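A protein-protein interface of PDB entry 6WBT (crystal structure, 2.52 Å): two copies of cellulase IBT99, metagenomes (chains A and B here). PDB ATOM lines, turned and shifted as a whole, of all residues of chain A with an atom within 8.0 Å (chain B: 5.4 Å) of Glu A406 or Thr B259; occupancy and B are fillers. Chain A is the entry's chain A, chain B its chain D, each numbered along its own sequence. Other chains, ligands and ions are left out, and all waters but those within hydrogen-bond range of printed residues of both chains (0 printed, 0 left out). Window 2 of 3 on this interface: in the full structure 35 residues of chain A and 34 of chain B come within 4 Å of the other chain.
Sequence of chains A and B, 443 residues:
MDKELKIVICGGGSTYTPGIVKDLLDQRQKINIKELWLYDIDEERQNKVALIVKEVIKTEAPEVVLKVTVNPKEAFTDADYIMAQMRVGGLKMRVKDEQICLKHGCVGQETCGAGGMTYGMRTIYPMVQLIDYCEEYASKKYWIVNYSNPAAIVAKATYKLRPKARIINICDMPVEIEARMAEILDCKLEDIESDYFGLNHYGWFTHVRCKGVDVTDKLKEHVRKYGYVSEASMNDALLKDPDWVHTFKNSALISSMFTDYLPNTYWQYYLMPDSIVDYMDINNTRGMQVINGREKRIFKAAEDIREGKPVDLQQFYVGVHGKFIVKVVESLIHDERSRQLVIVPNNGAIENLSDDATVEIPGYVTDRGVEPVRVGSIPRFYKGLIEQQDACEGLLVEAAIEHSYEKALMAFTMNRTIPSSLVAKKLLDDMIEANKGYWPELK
Of the 17 printed residues of chain A, 4 touch a printed residue of chain B. Hydrophobic or aromatic side chains of chain A within 4 Å of the printed part of chain B: Leu A409 and Met A410. Of the 9 printed residues of chain B, 4 touch a printed residue of chain A. Hydrophobic or aromatic side chains of chain B that line the printed part of chain A: Met B257 and Phe B258. Among the printed residues, 8 pairs touch across the chains. Among the printed residues, no Asp or Glu carboxylate lies within 4 Å of a Lys or Arg side-chain nitrogen of the other chain.
NZ of Lys B220 lies within hydrogen-bond range of O of Thr B259. NH2 of Arg B224 lies within hydrogen-bond range of O of Thr B259, 3.3 Å away. NZ of Lys B220 sits at hydrogen-bond distance from O of Asp B260 (2.8 Å). The backbone NH (N) of Glu A406 sits close to the side-chain hydroxyl (OG) of Ser A404. OG1 of Thr A413 sits at hydrogen-bond distance from O of Leu A409 (2.8 Å).
OG1 of Thr B259 is in hydrogen-bond range of OE2 of Glu A406, 2.8 Å away. OE1 of Glu A406 lies close to OD1 of Asp B260, 3.3 Å away.
Of chain B, only Met B257, Phe B258, Thr B259 and Asp B260 come within 4 Å of Glu A406. Of chain A, only Glu A406 comes within 4 Å of Thr B259. Of the printed residues of chain A, Met B257 touches Glu A406 and Leu A409. Of the printed residues of chain B, Thr A413 touches Phe B258. Of the printed residues of chain A, Asp B260 touches Glu A406 and Met A410. Tyr A405 touches none of the printed residues of chain B. Leu A395 touches none of the printed residues of chain B. The nearest residue of chain B that does not touch Glu A406 is Ser B256 (5.2 Å). The nearest printed residue of chain B that does not touch Met A410 is Thr B259 (5.3 Å).
No position is printed for both chains. Of the 8 pairs that touch across the chains among the printed residues, none has its exchanged pair printed and touching as well.
Met B257 touches Glu A406. Glu A406 touches Phe B258. Met B257 touches Leu A409 (CB to CD2, 3.7 Å). Phe B258 touches Met A410 (CE1 to CG, 3.6 Å). CE of Met A410 touches OD1 of Asp B260 (3.3 Å). Thr A413 touches Phe B258 (OG1 to CZ, 3.9 Å).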
ATOM      1  N   LEU A 395      15.726   6.092 -26.843  1.00  0.00           N
ATOM      2  CA  LEU A 395      16.819   5.126 -26.792  1.00  0.00           C
ATOM      3  C   LEU A 395      18.177   5.810 -26.871  1.00  0.00           C
ATOM      4  O   LEU A 395      19.159   5.301 -26.317  1.00  0.00           O
ATOM      5  CB  LEU A 395      16.674   4.106 -27.921  1.00  0.00           C
ATOM      6  CG  LEU A 395      15.501   3.129 -27.822  1.00  0.00           C
ATOM      7  CD1 LEU A 395      15.273   2.435 -29.154  1.00  0.00           C
ATOM      8  CD2 LEU A 395      15.741   2.111 -26.719  1.00  0.00           C
ATOM      9  N   ALA A 399      21.250   5.706 -24.118  1.00  0.00           N
ATOM     10  CA  ALA A 399      22.609   5.339 -24.502  1.00  0.00           C
ATOM     11  C   ALA A 399      23.641   6.262 -23.866  1.00  0.00           C
ATOM     12  O   ALA A 399      24.760   5.827 -23.570  1.00  0.00           O
ATOM     13  CB  ALA A 399      22.746   5.356 -26.024  1.00  0.00           C
ATOM     14  N   GLU A 402      23.329   5.220 -19.735  1.00  0.00           N
ATOM     15  CA  GLU A 402      23.766   3.871 -19.407  1.00  0.00           C
ATOM     16  C   GLU A 402      25.047   3.465 -20.122  1.00  0.00           C
ATOM     17  O   GLU A 402      25.546   2.359 -19.881  1.00  0.00           O
ATOM     18  CB  GLU A 402      22.650   2.874 -19.736  1.00  0.00           C
ATOM     19  CG  GLU A 402      21.331   3.201 -19.056  1.00  0.00           C
ATOM     20  CD  GLU A 402      20.144   2.565 -19.748  1.00  0.00           C
ATOM     21  OE1 GLU A 402      20.360   1.738 -20.659  1.00  0.00           O
ATOM     22  OE2 GLU A 402      18.997   2.896 -19.387  1.00  0.00           O
ATOM     23  N   HIS A 403      25.588   4.325 -20.990  1.00  0.00           N
ATOM     24  CA  HIS A 403      26.826   4.048 -21.721  1.00  0.00           C
ATOM     25  C   HIS A 403      26.724   2.747 -22.513  1.00  0.00           C
ATOM     26  O   HIS A 403      27.686   1.984 -22.618  1.00  0.00           O
ATOM     27  CB  HIS A 403      28.031   4.015 -20.776  1.00  0.00           C
ATOM     28  CG  HIS A 403      28.266   5.303 -20.051  1.00  0.00           C
ATOM     29  ND1 HIS A 403      29.163   6.252 -20.491  1.00  0.00           N
ATOM     30  CD2 HIS A 403      27.720   5.799 -18.916  1.00  0.00           C
ATOM     31  CE1 HIS A 403      29.160   7.277 -19.657  1.00  0.00           C
ATOM     32  NE2 HIS A 403      28.293   7.027 -18.693  1.00  0.00           N
ATOM     33  N   SER A 404      25.548   2.493 -23.078  1.00  0.00           N
ATOM     34  CA  SER A 404      25.257   1.239 -23.760  1.00  0.00           C
ATOM     35  C   SER A 404      25.404   1.427 -25.265  1.00  0.00           C
ATOM     36  O   SER A 404      24.719   2.265 -25.861  1.00  0.00           O
ATOM     37  CB  SER A 404      23.851   0.750 -23.413  1.00  0.00           C
ATOM     38  OG  SER A 404      23.517  -0.414 -24.148  1.00  0.00           O
ATOM     39  N   TYR A 405      26.298   0.644 -25.872  1.00  0.00           N
ATOM     40  CA  TYR A 405      26.439   0.660 -27.324  1.00  0.00           C
ATOM     41  C   TYR A 405      25.192   0.119 -28.010  1.00  0.00           C
ATOM     42  O   TYR A 405      24.833   0.583 -29.099  1.00  0.00           O
ATOM     43  CB  TYR A 405      27.672  -0.149 -27.735  1.00  0.00           C
ATOM     44  CG  TYR A 405      27.828  -0.351 -29.227  1.00  0.00           C
ATOM     45  CD1 TYR A 405      27.310  -1.478 -29.855  1.00  0.00           C
ATOM     46  CD2 TYR A 405      28.504   0.578 -30.007  1.00  0.00           C
ATOM     47  CE1 TYR A 405      27.451  -1.668 -31.215  1.00  0.00           C
ATOM     48  CE2 TYR A 405      28.653   0.395 -31.370  1.00  0.00           C
ATOM     49  CZ  TYR A 405      28.125  -0.729 -31.968  1.00  0.00           C
ATOM     50  OH  TYR A 405      28.268  -0.917 -33.323  1.00  0.00           O
ATOM     51  N   GLU A 406      24.522  -0.856 -27.393  1.00  0.00           N
ATOM     52  CA  GLU A 406      23.352  -1.464 -28.016  1.00  0.00           C
ATOM     53  C   GLU A 406      22.170  -0.505 -28.053  1.00  0.00           C
ATOM     54  O   GLU A 406      21.381  -0.534 -29.005  1.00  0.00           O
ATOM     55  CB  GLU A 406      22.974  -2.748 -27.276  1.00  0.00           C
ATOM     56  CG  GLU A 406      22.059  -3.669 -28.061  1.00  0.00           C
ATOM     57  CD  GLU A 406      21.829  -4.992 -27.359  1.00  0.00           C
ATOM     58  OE1 GLU A 406      20.655  -5.381 -27.186  1.00  0.00           O
ATOM     59  OE2 GLU A 406      22.825  -5.642 -26.975  1.00  0.00           O
ATOM     60  N   LYS A 407      22.030   0.347 -27.034  1.00  0.00           N
ATOM     61  CA  LYS A 407      20.968   1.348 -27.052  1.00  0.00           C
ATOM     62  C   LYS A 407      21.175   2.348 -28.181  1.00  0.00           C
ATOM     63  O   LYS A 407      20.208   2.823 -28.787  1.00  0.00           O
ATOM     64  CB  LYS A 407      20.902   2.069 -25.706  1.00  0.00           C
ATOM     65  CG  LYS A 407      20.498   1.187 -24.534  1.00  0.00           C
ATOM     66  CD  LYS A 407      18.995   1.194 -24.313  1.00  0.00           C
ATOM     67  CE  LYS A 407      18.622   0.399 -23.070  1.00  0.00           C
ATOM     68  NZ  LYS A 407      17.191   0.583 -22.696  1.00  0.00           N
ATOM     69  N   ALA A 408      22.434   2.682 -28.478  1.00  0.00           N
ATOM     70  CA  ALA A 408      22.717   3.579 -29.593  1.00  0.00           C
ATOM     71  C   ALA A 408      22.385   2.921 -30.925  1.00  0.00           C
ATOM     72  O   ALA A 408      21.843   3.570 -31.827  1.00  0.00           O
ATOM     73  CB  ALA A 408      24.181   4.019 -29.558  1.00  0.00           C
ATOM     74  N   LEU A 409      22.702   1.632 -31.068  1.00  0.00           N
ATOM     75  CA  LEU A 409      22.340   0.912 -32.285  1.00  0.00           C
ATOM     76  C   LEU A 409      20.827   0.828 -32.442  1.00  0.00           C
ATOM     77  O   LEU A 409      20.305   0.886 -33.561  1.00  0.00           O
ATOM     78  CB  LEU A 409      22.961  -0.485 -32.271  1.00  0.00           C
ATOM     79  CG  LEU A 409      22.689  -1.367 -33.489  1.00  0.00           C
ATOM     80  CD1 LEU A 409      23.221  -0.711 -34.753  1.00  0.00           C
ATOM     81  CD2 LEU A 409      23.299  -2.745 -33.297  1.00  0.00           C
ATOM     82  N   MET A 410      20.110   0.694 -31.331  1.00  0.00           N
ATOM     83  CA  MET A 410      18.654   0.677 -31.348  1.00  0.00           C
ATOM     84  C   MET A 410      18.099   2.039 -31.749  1.00  0.00           C
ATOM     85  O   MET A 410      17.055   2.131 -32.394  1.00  0.00           O
ATOM     86  CB  MET A 410      18.110   0.265 -29.980  1.00  0.00           C
ATOM     87  CG  MET A 410      18.272  -1.213 -29.667  1.00  0.00           C
ATOM     88  SD  MET A 410      17.679  -1.675 -27.870  1.00  0.00           S
ATOM     89  CE  MET A 410      17.688  -3.616 -28.039  1.00  0.00           C
ATOM     90  N   ALA A 411      18.811   3.100 -31.359  1.00  0.00           N
ATOM     91  CA  ALA A 411      18.382   4.447 -31.715  1.00  0.00           C
ATOM     92  C   ALA A 411      18.567   4.710 -33.205  1.00  0.00           C
ATOM     93  O   ALA A 411      17.716   5.343 -33.841  1.00  0.00           O
ATOM     94  CB  ALA A 411      19.146   5.480 -30.888  1.00  0.00           C
ATOM     95  N   PHE A 412      19.672   4.230 -33.778  1.00  0.00           N
ATOM     96  CA  PHE A 412      19.916   4.439 -35.202  1.00  0.00           C
ATOM     97  C   PHE A 412      19.022   3.547 -36.055  1.00  0.00           C
ATOM     98  O   PHE A 412      18.552   3.967 -37.119  1.00  0.00           O
ATOM     99  CB  PHE A 412      21.391   4.195 -35.522  1.00  0.00           C
ATOM    100  CG  PHE A 412      22.285   5.358 -35.191  1.00  0.00           C
ATOM    101  CD1 PHE A 412      22.429   5.791 -33.883  1.00  0.00           C
ATOM    102  CD2 PHE A 412      22.989   6.013 -36.188  1.00  0.00           C
ATOM    103  CE1 PHE A 412      23.251   6.859 -33.576  1.00  0.00           C
ATOM    104  CE2 PHE A 412      23.813   7.082 -35.887  1.00  0.00           C
ATOM    105  CZ  PHE A 412      23.945   7.505 -34.579  1.00  0.00           C
ATOM    106  N   THR A 413      18.772   2.314 -35.605  1.00  0.00           N
ATOM    107  CA  THR A 413      17.889   1.421 -36.349  1.00  0.00           C
ATOM    108  C   THR A 413      16.462   1.957 -36.397  1.00  0.00           C
ATOM    109  O   THR A 413      15.767   1.785 -37.406  1.00  0.00           O
ATOM    110  CB  THR A 413      17.913   0.023 -35.723  1.00  0.00           C
ATOM    111  OG1 THR A 413      19.250  -0.495 -35.754  1.00  0.00           O
ATOM    112  CG2 THR A 413      16.991  -0.926 -36.475  1.00  0.00           C
ATOM    113  N   LEU A 428      26.785   4.096 -37.059  1.00  0.00           N
ATOM    114  CA  LEU A 428      27.074   4.298 -35.643  1.00  0.00           C
ATOM    115  C   LEU A 428      28.568   4.191 -35.366  1.00  0.00           C
ATOM    116  O   LEU A 428      29.157   5.071 -34.728  1.00  0.00           O
ATOM    117  CB  LEU A 428      26.297   3.289 -34.796  1.00  0.00           C
ATOM    118  CG  LEU A 428      26.545   3.339 -33.287  1.00  0.00           C
ATOM    119  CD1 LEU A 428      26.153   4.694 -32.720  1.00  0.00           C
ATOM    120  CD2 LEU A 428      25.792   2.222 -32.582  1.00  0.00           C
ATOM    121  N   LEU A 442      30.822   4.160 -24.905  1.00  0.00           N
ATOM    122  CA  LEU A 442      29.752   3.199 -25.156  1.00  0.00           C
ATOM    123  C   LEU A 442      30.341   1.795 -25.138  1.00  0.00           C
ATOM    124  O   LEU A 442      31.093   1.420 -26.044  1.00  0.00           O
ATOM    125  CB  LEU A 442      29.057   3.481 -26.489  1.00  0.00           C
ATOM    126  CG  LEU A 442      28.338   4.828 -26.604  1.00  0.00           C
ATOM    127  CD1 LEU A 442      27.620   4.942 -27.940  1.00  0.00           C
ATOM    128  CD2 LEU A 442      27.366   5.016 -25.451  1.00  0.00           C
ATOM    129  N   LYS A 443      29.999   1.023 -24.111  1.00  0.00           N
ATOM    130  CA  LYS A 443      30.443  -0.363 -24.011  1.00  0.00           C
ATOM    131  C   LYS A 443      29.354  -1.314 -24.493  1.00  0.00           C
ATOM    132  O   LYS A 443      28.167  -1.076 -24.273  1.00  0.00           O
ATOM    133  CB  LYS A 443      30.839  -0.703 -22.572  1.00  0.00           C
ATOM    134  CG  LYS A 443      32.098  -0.003 -22.086  1.00  0.00           C
ATOM    135  CD  LYS A 443      32.480  -0.475 -20.691  1.00  0.00           C
ATOM    136  CE  LYS A 443      33.769   0.175 -20.217  1.00  0.00           C
ATOM    137  NZ  LYS A 443      34.919  -0.154 -21.104  1.00  0.00           N
ATOM    138  N   LYS B 220      20.281 -18.664 -27.604  1.00  0.00           N
ATOM    139  CA  LYS B 220      20.832 -17.473 -28.242  1.00  0.00           C
ATOM    140  C   LYS B 220      22.337 -17.571 -28.452  1.00  0.00           C
ATOM    141  O   LYS B 220      22.875 -16.869 -29.313  1.00  0.00           O
ATOM    142  CB  LYS B 220      20.483 -16.228 -27.422  1.00  0.00           C
ATOM    143  CG  LYS B 220      21.034 -16.215 -26.007  1.00  0.00           C
ATOM    144  CD  LYS B 220      20.130 -15.414 -25.075  1.00  0.00           C
ATOM    145  CE  LYS B 220      19.717 -14.088 -25.696  1.00  0.00           C
ATOM    146  NZ  LYS B 220      18.845 -13.289 -24.790  1.00  0.00           N
ATOM    147  N   ARG B 224      22.988 -17.076 -32.418  1.00  0.00           N
ATOM    148  CA  ARG B 224      23.869 -16.001 -32.859  1.00  0.00           C
ATOM    149  C   ARG B 224      24.973 -16.495 -33.785  1.00  0.00           C
ATOM    150  O   ARG B 224      25.589 -15.682 -34.480  1.00  0.00           O
ATOM    151  CB  ARG B 224      24.487 -15.290 -31.653  1.00  0.00           C
ATOM    152  CG  ARG B 224      23.556 -14.308 -30.967  1.00  0.00           C
ATOM    153  CD  ARG B 224      24.076 -13.938 -29.590  1.00  0.00           C
ATOM    154  NE  ARG B 224      23.089 -13.193 -28.817  1.00  0.00           N
ATOM    155  CZ  ARG B 224      23.128 -13.052 -27.496  1.00  0.00           C
ATOM    156  NH1 ARG B 224      24.104 -13.615 -26.796  1.00  0.00           N
ATOM    157  NH2 ARG B 224      22.188 -12.356 -26.875  1.00  0.00           N
ATOM    158  N   SER B 255      19.823 -11.539 -33.844  1.00  0.00           N
ATOM    159  CA  SER B 255      20.000 -11.984 -32.467  1.00  0.00           C
ATOM    160  C   SER B 255      21.307 -11.489 -31.862  1.00  0.00           C
ATOM    161  O   SER B 255      21.439 -11.472 -30.634  1.00  0.00           O
ATOM    162  CB  SER B 255      19.940 -13.510 -32.393  1.00  0.00           C
ATOM    163  OG  SER B 255      20.976 -14.099 -33.159  1.00  0.00           O
ATOM    164  N   SER B 256      22.271 -11.087 -32.690  1.00  0.00           N
ATOM    165  CA  SER B 256      23.549 -10.594 -32.196  1.00  0.00           C
ATOM    166  C   SER B 256      23.547  -9.091 -31.954  1.00  0.00           C
ATOM    167  O   SER B 256      24.193  -8.625 -31.009  1.00  0.00           O
ATOM    168  CB  SER B 256      24.667 -10.950 -33.179  1.00  0.00           C
ATOM    169  OG  SER B 256      24.735 -12.351 -33.389  1.00  0.00           O
ATOM    170  N   MET B 257      22.841  -8.327 -32.781  1.00  0.00           N
ATOM    171  CA  MET B 257      22.787  -6.878 -32.628  1.00  0.00           C
ATOM    172  C   MET B 257      21.887  -6.467 -31.468  1.00  0.00           C
ATOM    173  O   MET B 257      22.104  -5.431 -30.838  1.00  0.00           O
ATOM    174  CB  MET B 257      22.301  -6.221 -33.923  1.00  0.00           C
ATOM    175  CG  MET B 257      23.327  -6.225 -35.043  1.00  0.00           C
ATOM    176  SD  MET B 257      22.684  -5.319 -36.645  1.00  0.00           S
ATOM    177  CE  MET B 257      24.343  -5.301 -37.667  1.00  0.00           C
ATOM    178  N   PHE B 258      20.874  -7.284 -31.191  1.00  0.00           N
ATOM    179  CA  PHE B 258      19.926  -7.035 -30.109  1.00  0.00           C
ATOM    180  C   PHE B 258      19.882  -8.283 -29.238  1.00  0.00           C
ATOM    181  O   PHE B 258      19.359  -9.320 -29.657  1.00  0.00           O
ATOM    182  CB  PHE B 258      18.546  -6.682 -30.660  1.00  0.00           C
ATOM    183  CG  PHE B 258      18.582  -5.654 -31.757  1.00  0.00           C
ATOM    184  CD1 PHE B 258      18.788  -4.315 -31.465  1.00  0.00           C
ATOM    185  CD2 PHE B 258      18.421  -6.027 -33.082  1.00  0.00           C
ATOM    186  CE1 PHE B 258      18.828  -3.367 -32.473  1.00  0.00           C
ATOM    187  CE2 PHE B 258      18.458  -5.084 -34.093  1.00  0.00           C
ATOM    188  CZ  PHE B 258      18.663  -3.753 -33.788  1.00  0.00           C
ATOM    189  N   THR B 259      20.429  -8.180 -28.027  1.00  0.00           N
ATOM    190  CA  THR B 259      20.740  -9.338 -27.200  1.00  0.00           C
ATOM    191  C   THR B 259      19.657  -9.677 -26.183  1.00  0.00           C
ATOM    192  O   THR B 259      19.830 -10.631 -25.419  1.00  0.00           O
ATOM    193  CB  THR B 259      22.065  -9.111 -26.465  1.00  0.00           C
ATOM    194  OG1 THR B 259      21.950  -7.967 -25.610  1.00  0.00           O
ATOM    195  CG2 THR B 259      23.192  -8.882 -27.461  1.00  0.00           C
ATOM    196  N   ASP B 260      18.551  -8.934 -26.151  1.00  0.00           N
ATOM    197  CA  ASP B 260      17.534  -9.181 -25.133  1.00  0.00           C
ATOM    198  C   ASP B 260      16.774 -10.473 -25.413  1.00  0.00           C
ATOM    199  O   ASP B 260      16.791 -11.408 -24.603  1.00  0.00           O
ATOM    200  CB  ASP B 260      16.570  -7.997 -25.050  1.00  0.00           C
ATOM    201  CG  ASP B 260      17.282  -6.676 -24.842  1.00  0.00           C
ATOM    202  OD1 ASP B 260      17.677  -6.050 -25.846  1.00  0.00           O
ATOM    203  OD2 ASP B 260      17.451  -6.267 -23.674  1.00  0.00           O
ATOM    204  N   TYR B 261      16.102 -10.544 -26.557  1.00  0.00           N
ATOM    205  CA  TYR B 261      15.191 -11.635 -26.868  1.00  0.00           C
ATOM    206  C   TYR B 261      15.653 -12.379 -28.115  1.00  0.00           C
ATOM    207  O   TYR B 261      16.516 -11.916 -28.866  1.00  0.00           O
ATOM    208  CB  TYR B 261      13.764 -11.110 -27.073  1.00  0.00           C
ATOM    209  CG  TYR B 261      13.291 -10.167 -25.991  1.00  0.00           C
ATOM    210  CD1 TYR B 261      13.526 -10.441 -24.650  1.00  0.00           C
ATOM    211  CD2 TYR B 261      12.615  -8.997 -26.313  1.00  0.00           C
ATOM    212  CE1 TYR B 261      13.097  -9.578 -23.660  1.00  0.00           C
ATOM    213  CE2 TYR B 261      12.183  -8.129 -25.330  1.00  0.00           C
ATOM    214  CZ  TYR B 261      12.426  -8.424 -24.005  1.00  0.00           C
ATOM    215  OH  TYR B 261      11.997  -7.562 -23.023  1.00  0.00           O
